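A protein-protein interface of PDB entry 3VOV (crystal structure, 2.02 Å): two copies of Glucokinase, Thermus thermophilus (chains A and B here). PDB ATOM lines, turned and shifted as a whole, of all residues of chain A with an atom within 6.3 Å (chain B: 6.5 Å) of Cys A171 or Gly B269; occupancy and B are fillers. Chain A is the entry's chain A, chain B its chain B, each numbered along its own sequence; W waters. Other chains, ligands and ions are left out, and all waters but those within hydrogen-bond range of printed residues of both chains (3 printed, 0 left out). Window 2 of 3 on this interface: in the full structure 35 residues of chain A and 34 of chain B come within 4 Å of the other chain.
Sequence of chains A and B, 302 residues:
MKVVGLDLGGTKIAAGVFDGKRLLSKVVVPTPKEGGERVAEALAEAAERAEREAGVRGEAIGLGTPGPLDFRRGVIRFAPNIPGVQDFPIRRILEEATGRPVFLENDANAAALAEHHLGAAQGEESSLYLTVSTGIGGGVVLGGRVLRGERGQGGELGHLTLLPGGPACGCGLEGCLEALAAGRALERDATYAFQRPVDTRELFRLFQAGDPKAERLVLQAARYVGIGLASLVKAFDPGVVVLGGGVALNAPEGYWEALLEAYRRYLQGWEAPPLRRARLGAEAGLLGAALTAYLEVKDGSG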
ATOM      1  N   GLN A 153     -13.153 -16.544 -11.655  1.00  0.00           N
ATOM      2  CA  GLN A 153     -13.353 -16.639 -10.200  1.00  0.00           C
ATOM      3  C   GLN A 153     -14.761 -16.194  -9.755  1.00  0.00           C
ATOM      4  O   GLN A 153     -15.039 -16.150  -8.548  1.00  0.00           O
ATOM      5  CB  GLN A 153     -12.339 -15.774  -9.396  1.00  0.00           C
ATOM      6  CG  GLN A 153     -10.872 -16.004  -9.638  1.00  0.00           C
ATOM      7  CD  GLN A 153      -9.980 -15.030  -8.835  1.00  0.00           C
ATOM      8  OE1 GLN A 153      -9.033 -15.466  -8.142  1.00  0.00           O
ATOM      9  NE2 GLN A 153     -10.279 -13.696  -8.926  1.00  0.00           N
ATOM     10  N   HIS A 159     -16.379 -18.392  -0.425  1.00  0.00           N
ATOM     11  CA  HIS A 159     -15.239 -17.651   0.091  1.00  0.00           C
ATOM     12  C   HIS A 159     -15.489 -16.193   0.394  1.00  0.00           C
ATOM     13  O   HIS A 159     -14.542 -15.423   0.558  1.00  0.00           O
ATOM     14  CB  HIS A 159     -13.947 -17.922  -0.707  1.00  0.00           C
ATOM     15  CG  HIS A 159     -13.632 -19.388  -0.781  1.00  0.00           C
ATOM     16  ND1 HIS A 159     -13.060 -20.075   0.265  1.00  0.00           N
ATOM     17  CD2 HIS A 159     -13.962 -20.322  -1.706  1.00  0.00           C
ATOM     18  CE1 HIS A 159     -12.976 -21.361  -0.042  1.00  0.00           C
ATOM     19  NE2 HIS A 159     -13.533 -21.541  -1.231  1.00  0.00           N
ATOM     20  N   CYS A 169      -9.207 -20.921   6.415  1.00  0.00           N
ATOM     21  CA  CYS A 169      -9.822 -21.541   5.248  1.00  0.00           C
ATOM     22  C   CYS A 169      -8.769 -22.204   4.349  1.00  0.00           C
ATOM     23  O   CYS A 169      -7.623 -21.765   4.301  1.00  0.00           O
ATOM     24  CB  CYS A 169     -10.553 -20.484   4.390  1.00  0.00           C
ATOM     25  SG  CYS A 169     -11.633 -21.250   3.093  1.00  0.00           S
ATOM     26  N   GLY A 170      -9.177 -23.254   3.646  1.00  0.00           N
ATOM     27  CA  GLY A 170      -8.354 -23.903   2.624  1.00  0.00           C
ATOM     28  C   GLY A 170      -7.893 -22.934   1.547  1.00  0.00           C
ATOM     29  O   GLY A 170      -6.844 -23.155   0.930  1.00  0.00           O
ATOM     30  N   CYS A 171      -8.630 -21.835   1.324  1.00  0.00           N
ATOM     31  CA  CYS A 171      -8.273 -20.930   0.214  1.00  0.00           C
ATOM     32  C   CYS A 171      -7.084 -20.041   0.535  1.00  0.00           C
ATOM     33  O   CYS A 171      -6.447 -19.511  -0.370  1.00  0.00           O
ATOM     34  CB  CYS A 171      -9.454 -20.094  -0.284  1.00  0.00           C
ATOM     35  SG  CYS A 171      -9.863 -18.741   0.893  1.00  0.00           S
ATOM     36  N   GLY A 172      -6.786 -19.886   1.819  1.00  0.00           N
ATOM     37  CA  GLY A 172      -5.672 -19.045   2.254  1.00  0.00           C
ATOM     38  C   GLY A 172      -6.177 -17.891   3.127  1.00  0.00           C
ATOM     39  O   GLY A 172      -5.367 -17.173   3.717  1.00  0.00           O
ATOM     40  N   LEU A 173      -7.496 -17.711   3.216  1.00  0.00           N
ATOM     41  CA  LEU A 173      -8.066 -16.694   4.123  1.00  0.00           C
ATOM     42  C   LEU A 173      -8.531 -17.322   5.472  1.00  0.00           C
ATOM     43  O   LEU A 173      -8.064 -18.392   5.837  1.00  0.00           O
ATOM     44  CB  LEU A 173      -9.230 -15.932   3.454  1.00  0.00           C
ATOM     45  CG  LEU A 173      -8.932 -15.477   2.034  1.00  0.00           C
ATOM     46  CD1 LEU A 173     -10.185 -14.748   1.391  1.00  0.00           C
ATOM     47  CD2 LEU A 173      -7.680 -14.630   2.022  1.00  0.00           C
ATOM     48  N   GLU A 174      -9.461 -16.661   6.159  1.00  0.00           N
ATOM     49  CA  GLU A 174     -10.045 -17.174   7.404  1.00  0.00           C
ATOM     50  C   GLU A 174     -11.448 -16.587   7.510  1.00  0.00           C
ATOM     51  O   GLU A 174     -11.698 -15.498   6.980  1.00  0.00           O
ATOM     52  CB  GLU A 174      -9.173 -16.797   8.641  1.00  0.00           C
ATOM     53  CG  GLU A 174      -9.506 -15.466   9.398  1.00  0.00           C
ATOM     54  CD  GLU A 174      -9.318 -14.172   8.598  1.00  0.00           C
ATOM     55  OE1 GLU A 174      -8.488 -14.109   7.655  1.00  0.00           O
ATOM     56  OE2 GLU A 174      -9.931 -13.144   8.987  1.00  0.00           O
ATOM     57  N   CYS A 176     -14.134 -17.541   6.046  1.00  0.00           N
ATOM     58  CA  CYS A 176     -14.931 -17.760   4.833  1.00  0.00           C
ATOM     59  C   CYS A 176     -16.144 -18.555   5.231  1.00  0.00           C
ATOM     60  O   CYS A 176     -16.069 -19.402   6.119  1.00  0.00           O
ATOM     61  CB  CYS A 176     -14.133 -18.607   3.832  1.00  0.00           C
ATOM     62  SG  CYS A 176     -12.815 -17.690   3.096  1.00  0.00           S
ATOM     63  N   GLU A 178     -17.246 -21.108   3.646  1.00  0.00           N
ATOM     64  CA  GLU A 178     -16.817 -22.539   3.615  1.00  0.00           C
ATOM     65  C   GLU A 178     -16.107 -22.985   4.926  1.00  0.00           C
ATOM     66  O   GLU A 178     -16.418 -24.049   5.503  1.00  0.00           O
ATOM     67  CB  GLU A 178     -15.948 -22.816   2.393  1.00  0.00           C
ATOM     68  CG  GLU A 178     -15.181 -24.160   2.419  1.00  0.00           C
ATOM     69  CD  GLU A 178     -14.506 -24.478   1.082  1.00  0.00           C
ATOM     70  OE1 GLU A 178     -15.217 -24.825   0.102  1.00  0.00           O
ATOM     71  OE2 GLU A 178     -13.274 -24.414   1.009  1.00  0.00           O
ATOM     72  N   LYS B 234     -14.782 -12.136  -4.667  1.00  0.00           N
ATOM     73  CA  LYS B 234     -15.085 -13.573  -4.744  1.00  0.00           C
ATOM     74  C   LYS B 234     -16.462 -13.778  -5.398  1.00  0.00           C
ATOM     75  O   LYS B 234     -16.728 -14.786  -6.051  1.00  0.00           O
ATOM     76  CB  LYS B 234     -15.129 -14.208  -3.331  1.00  0.00           C
ATOM     77  CG  LYS B 234     -13.964 -13.847  -2.388  1.00  0.00           C
ATOM     78  CD  LYS B 234     -12.643 -14.280  -2.923  1.00  0.00           C
ATOM     79  CE  LYS B 234     -11.571 -14.142  -1.822  1.00  0.00           C
ATOM     80  NZ  LYS B 234     -11.563 -12.817  -1.091  1.00  0.00           N
ATOM     81  N   ARG B 264      -5.355  -6.632  -0.087  1.00  0.00           N
ATOM     82  CA  ARG B 264      -4.348  -7.627  -0.483  1.00  0.00           C
ATOM     83  C   ARG B 264      -4.312  -8.840   0.451  1.00  0.00           C
ATOM     84  O   ARG B 264      -4.278  -9.972  -0.032  1.00  0.00           O
ATOM     85  CB  ARG B 264      -2.984  -6.986  -0.555  1.00  0.00           C
ATOM     86  CG  ARG B 264      -2.902  -6.081  -1.782  1.00  0.00           C
ATOM     87  CD  ARG B 264      -1.511  -5.490  -1.882  1.00  0.00           C
ATOM     88  NE  ARG B 264      -1.395  -4.644  -3.065  1.00  0.00           N
ATOM     89  CZ  ARG B 264      -0.772  -3.469  -3.070  1.00  0.00           C
ATOM     90  NH1 ARG B 264      -0.256  -2.993  -1.935  1.00  0.00           N
ATOM     91  NH2 ARG B 264      -0.708  -2.758  -4.199  1.00  0.00           N
ATOM     92  N   LEU B 267      -7.060 -11.289  -0.280  1.00  0.00           N
ATOM     93  CA  LEU B 267      -6.923 -11.888  -1.584  1.00  0.00           C
ATOM     94  C   LEU B 267      -5.655 -12.765  -1.701  1.00  0.00           C
ATOM     95  O   LEU B 267      -5.275 -13.161  -2.828  1.00  0.00           O
ATOM     96  CB  LEU B 267      -6.978 -10.806  -2.648  1.00  0.00           C
ATOM     97  CG  LEU B 267      -8.376 -10.183  -2.861  1.00  0.00           C
ATOM     98  CD1 LEU B 267      -8.280  -8.876  -3.695  1.00  0.00           C
ATOM     99  CD2 LEU B 267      -9.306 -11.243  -3.558  1.00  0.00           C
ATOM    100  N   GLN B 268      -5.001 -13.064  -0.560  1.00  0.00           N
ATOM    101  CA  GLN B 268      -4.003 -14.163  -0.468  1.00  0.00           C
ATOM    102  C   GLN B 268      -4.690 -15.464  -0.898  1.00  0.00           C
ATOM    103  O   GLN B 268      -5.710 -15.873  -0.313  1.00  0.00           O
ATOM    104  CB  GLN B 268      -3.465 -14.326   0.962  1.00  0.00           C
ATOM    105  CG  GLN B 268      -2.544 -13.194   1.375  1.00  0.00           C
ATOM    106  CD  GLN B 268      -2.139 -13.188   2.873  1.00  0.00           C
ATOM    107  OE1 GLN B 268      -1.605 -12.175   3.330  1.00  0.00           O
ATOM    108  NE2 GLN B 268      -2.397 -14.292   3.631  1.00  0.00           N
ATOM    109  N   GLY B 269      -4.134 -16.101  -1.918  1.00  0.00           N
ATOM    110  CA  GLY B 269      -4.712 -17.327  -2.472  1.00  0.00           C
ATOM    111  C   GLY B 269      -5.593 -17.065  -3.692  1.00  0.00           C
ATOM    112  O   GLY B 269      -6.192 -18.023  -4.263  1.00  0.00           O
ATOM    113  N   TRP B 270      -5.661 -15.794  -4.097  1.00  0.00           N
ATOM    114  CA  TRP B 270      -6.594 -15.340  -5.141  1.00  0.00           C
ATOM    115  C   TRP B 270      -5.900 -14.402  -6.122  1.00  0.00           C
ATOM    116  O   TRP B 270      -4.870 -13.840  -5.790  1.00  0.00           O
ATOM    117  CB  TRP B 270      -7.792 -14.600  -4.480  1.00  0.00           C
ATOM    118  CG  TRP B 270      -8.573 -15.503  -3.591  1.00  0.00           C
ATOM    119  CD1 TRP B 270      -8.301 -15.817  -2.275  1.00  0.00           C
ATOM    120  CD2 TRP B 270      -9.748 -16.237  -3.945  1.00  0.00           C
ATOM    121  NE1 TRP B 270      -9.227 -16.720  -1.817  1.00  0.00           N
ATOM    122  CE2 TRP B 270     -10.133 -16.981  -2.812  1.00  0.00           C
ATOM    123  CE3 TRP B 270     -10.501 -16.365  -5.137  1.00  0.00           C
ATOM    124  CZ2 TRP B 270     -11.247 -17.841  -2.819  1.00  0.00           C
ATOM    125  CZ3 TRP B 270     -11.629 -17.207  -5.130  1.00  0.00           C
ATOM    126  CH2 TRP B 270     -11.985 -17.925  -3.977  1.00  0.00           C
ATOM    127  N   GLU B 271      -6.454 -14.248  -7.323  1.00  0.00           N
ATOM    128  CA  GLU B 271      -5.992 -13.202  -8.243  1.00  0.00           C
ATOM    129  C   GLU B 271      -6.711 -11.883  -7.898  1.00  0.00           C
ATOM    130  O   GLU B 271      -7.938 -11.785  -7.999  1.00  0.00           O
ATOM    131  CB  GLU B 271      -6.304 -13.544  -9.715  1.00  0.00           C
ATOM    132  CG  GLU B 271      -5.543 -14.694 -10.357  1.00  0.00           C
ATOM    133  CD  GLU B 271      -6.034 -14.957 -11.822  1.00  0.00           C
ATOM    134  OE1 GLU B 271      -6.740 -15.976 -12.019  1.00  0.00           O
ATOM    135  OE2 GLU B 271      -5.740 -14.144 -12.762  1.00  0.00           O
HETATM  136  O   HOH W   1     -13.427 -13.016   0.899  1.00  0.00           O
HETATM  137  O   HOH W   2      -2.744 -17.142   3.393  1.00  0.00           O
HETATM  138  O   HOH W   3      -6.690 -20.237  -3.128  1.00  0.00           O
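Hydrophobic or aromatic side chains of chain A that line the printed part of chain B: His A159 and Leu A173. Hydrophobic or aromatic side chains of chain B that line the printed part of chain A: Trp B270. Among the printed residues, 11 pairs touch across the chains.
No position is printed for both chains. Of the 11 pairs that touch across the chains among the printed residues, none has its exchanged pair printed and touching as well.
Printed residues of chain B within 4 Å of Gln A153: Lys B234 (3.3 Å), Trp B270 (3.5 Å) and Glu B271 (3.0 Å). Of chain B, only Gln B268, Gly B269 and Trp B270 come within 4 Å of Cys A171. Printed residues of chain B within 4 Å of Leu A173: Lys B234, Gln B268 and Trp B270. Of the printed residues of chain A, Lys B234 touches Gln A153, His A159 and Leu A173. Printed residues of chain A within 4 Å of Gln B268: Cys A171 and Leu A173. Of the printed residues of chain A, Trp B270 touches Gln A153, His A159, Cys A171 and Leu A173. The nearest residue of chain B that does not touch Cys A171 is Lys B234 (5.6 Å). The nearest residue of chain A that does not touch Gly B269 is Gly A172 (5.1 Å). The nearest printed residue of chain B that does not touch Leu A173 is Leu B267 (4.1 Å).
Trp B270 touches Gln A153 (CE3 to OE1, 3.5 Å). Lys B234 touches His A159. Trp B270 touches His A159 (CZ2 to CB, 3.4 Å). O of Cys A171 touches O of Gln B268 (3.7 Å). Cys A171 touches Gly B269 (O to CA, 3.5 Å). Lys B234 touches Leu A173. Gln B268 touches Leu A173 (O to CD2, 3.3 Å). CD1 of Leu A173 touches NE1 of Trp B270, 3.9 Å away.
N of Leu A173 sits close to SG of Cys A171, 3.5 Å away.
Water W3 bridges O of Gly B269 (2.5 Å) and O of Cys A171 (2.9 Å). Water W2 lies within hydrogen-bond range of O of Gly A172 (2.6 Å) and NE2 of Gln B268 (2.9 Å). Water W1 lies within hydrogen-bond range of the backbone carbonyl oxygen of His A159 (2.7 Å) and the side-chain amino group of Lys B234 (2.7 Å).
OE1 of Gln A153 lies within hydrogen-bond range of N of Glu B271, 3.0 Å away. SG of Cys A171 lies close to NE1 of Trp B270, at 3.4 Å. O of Lys B234 sits close to O of Gln A153 (3.3 Å).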
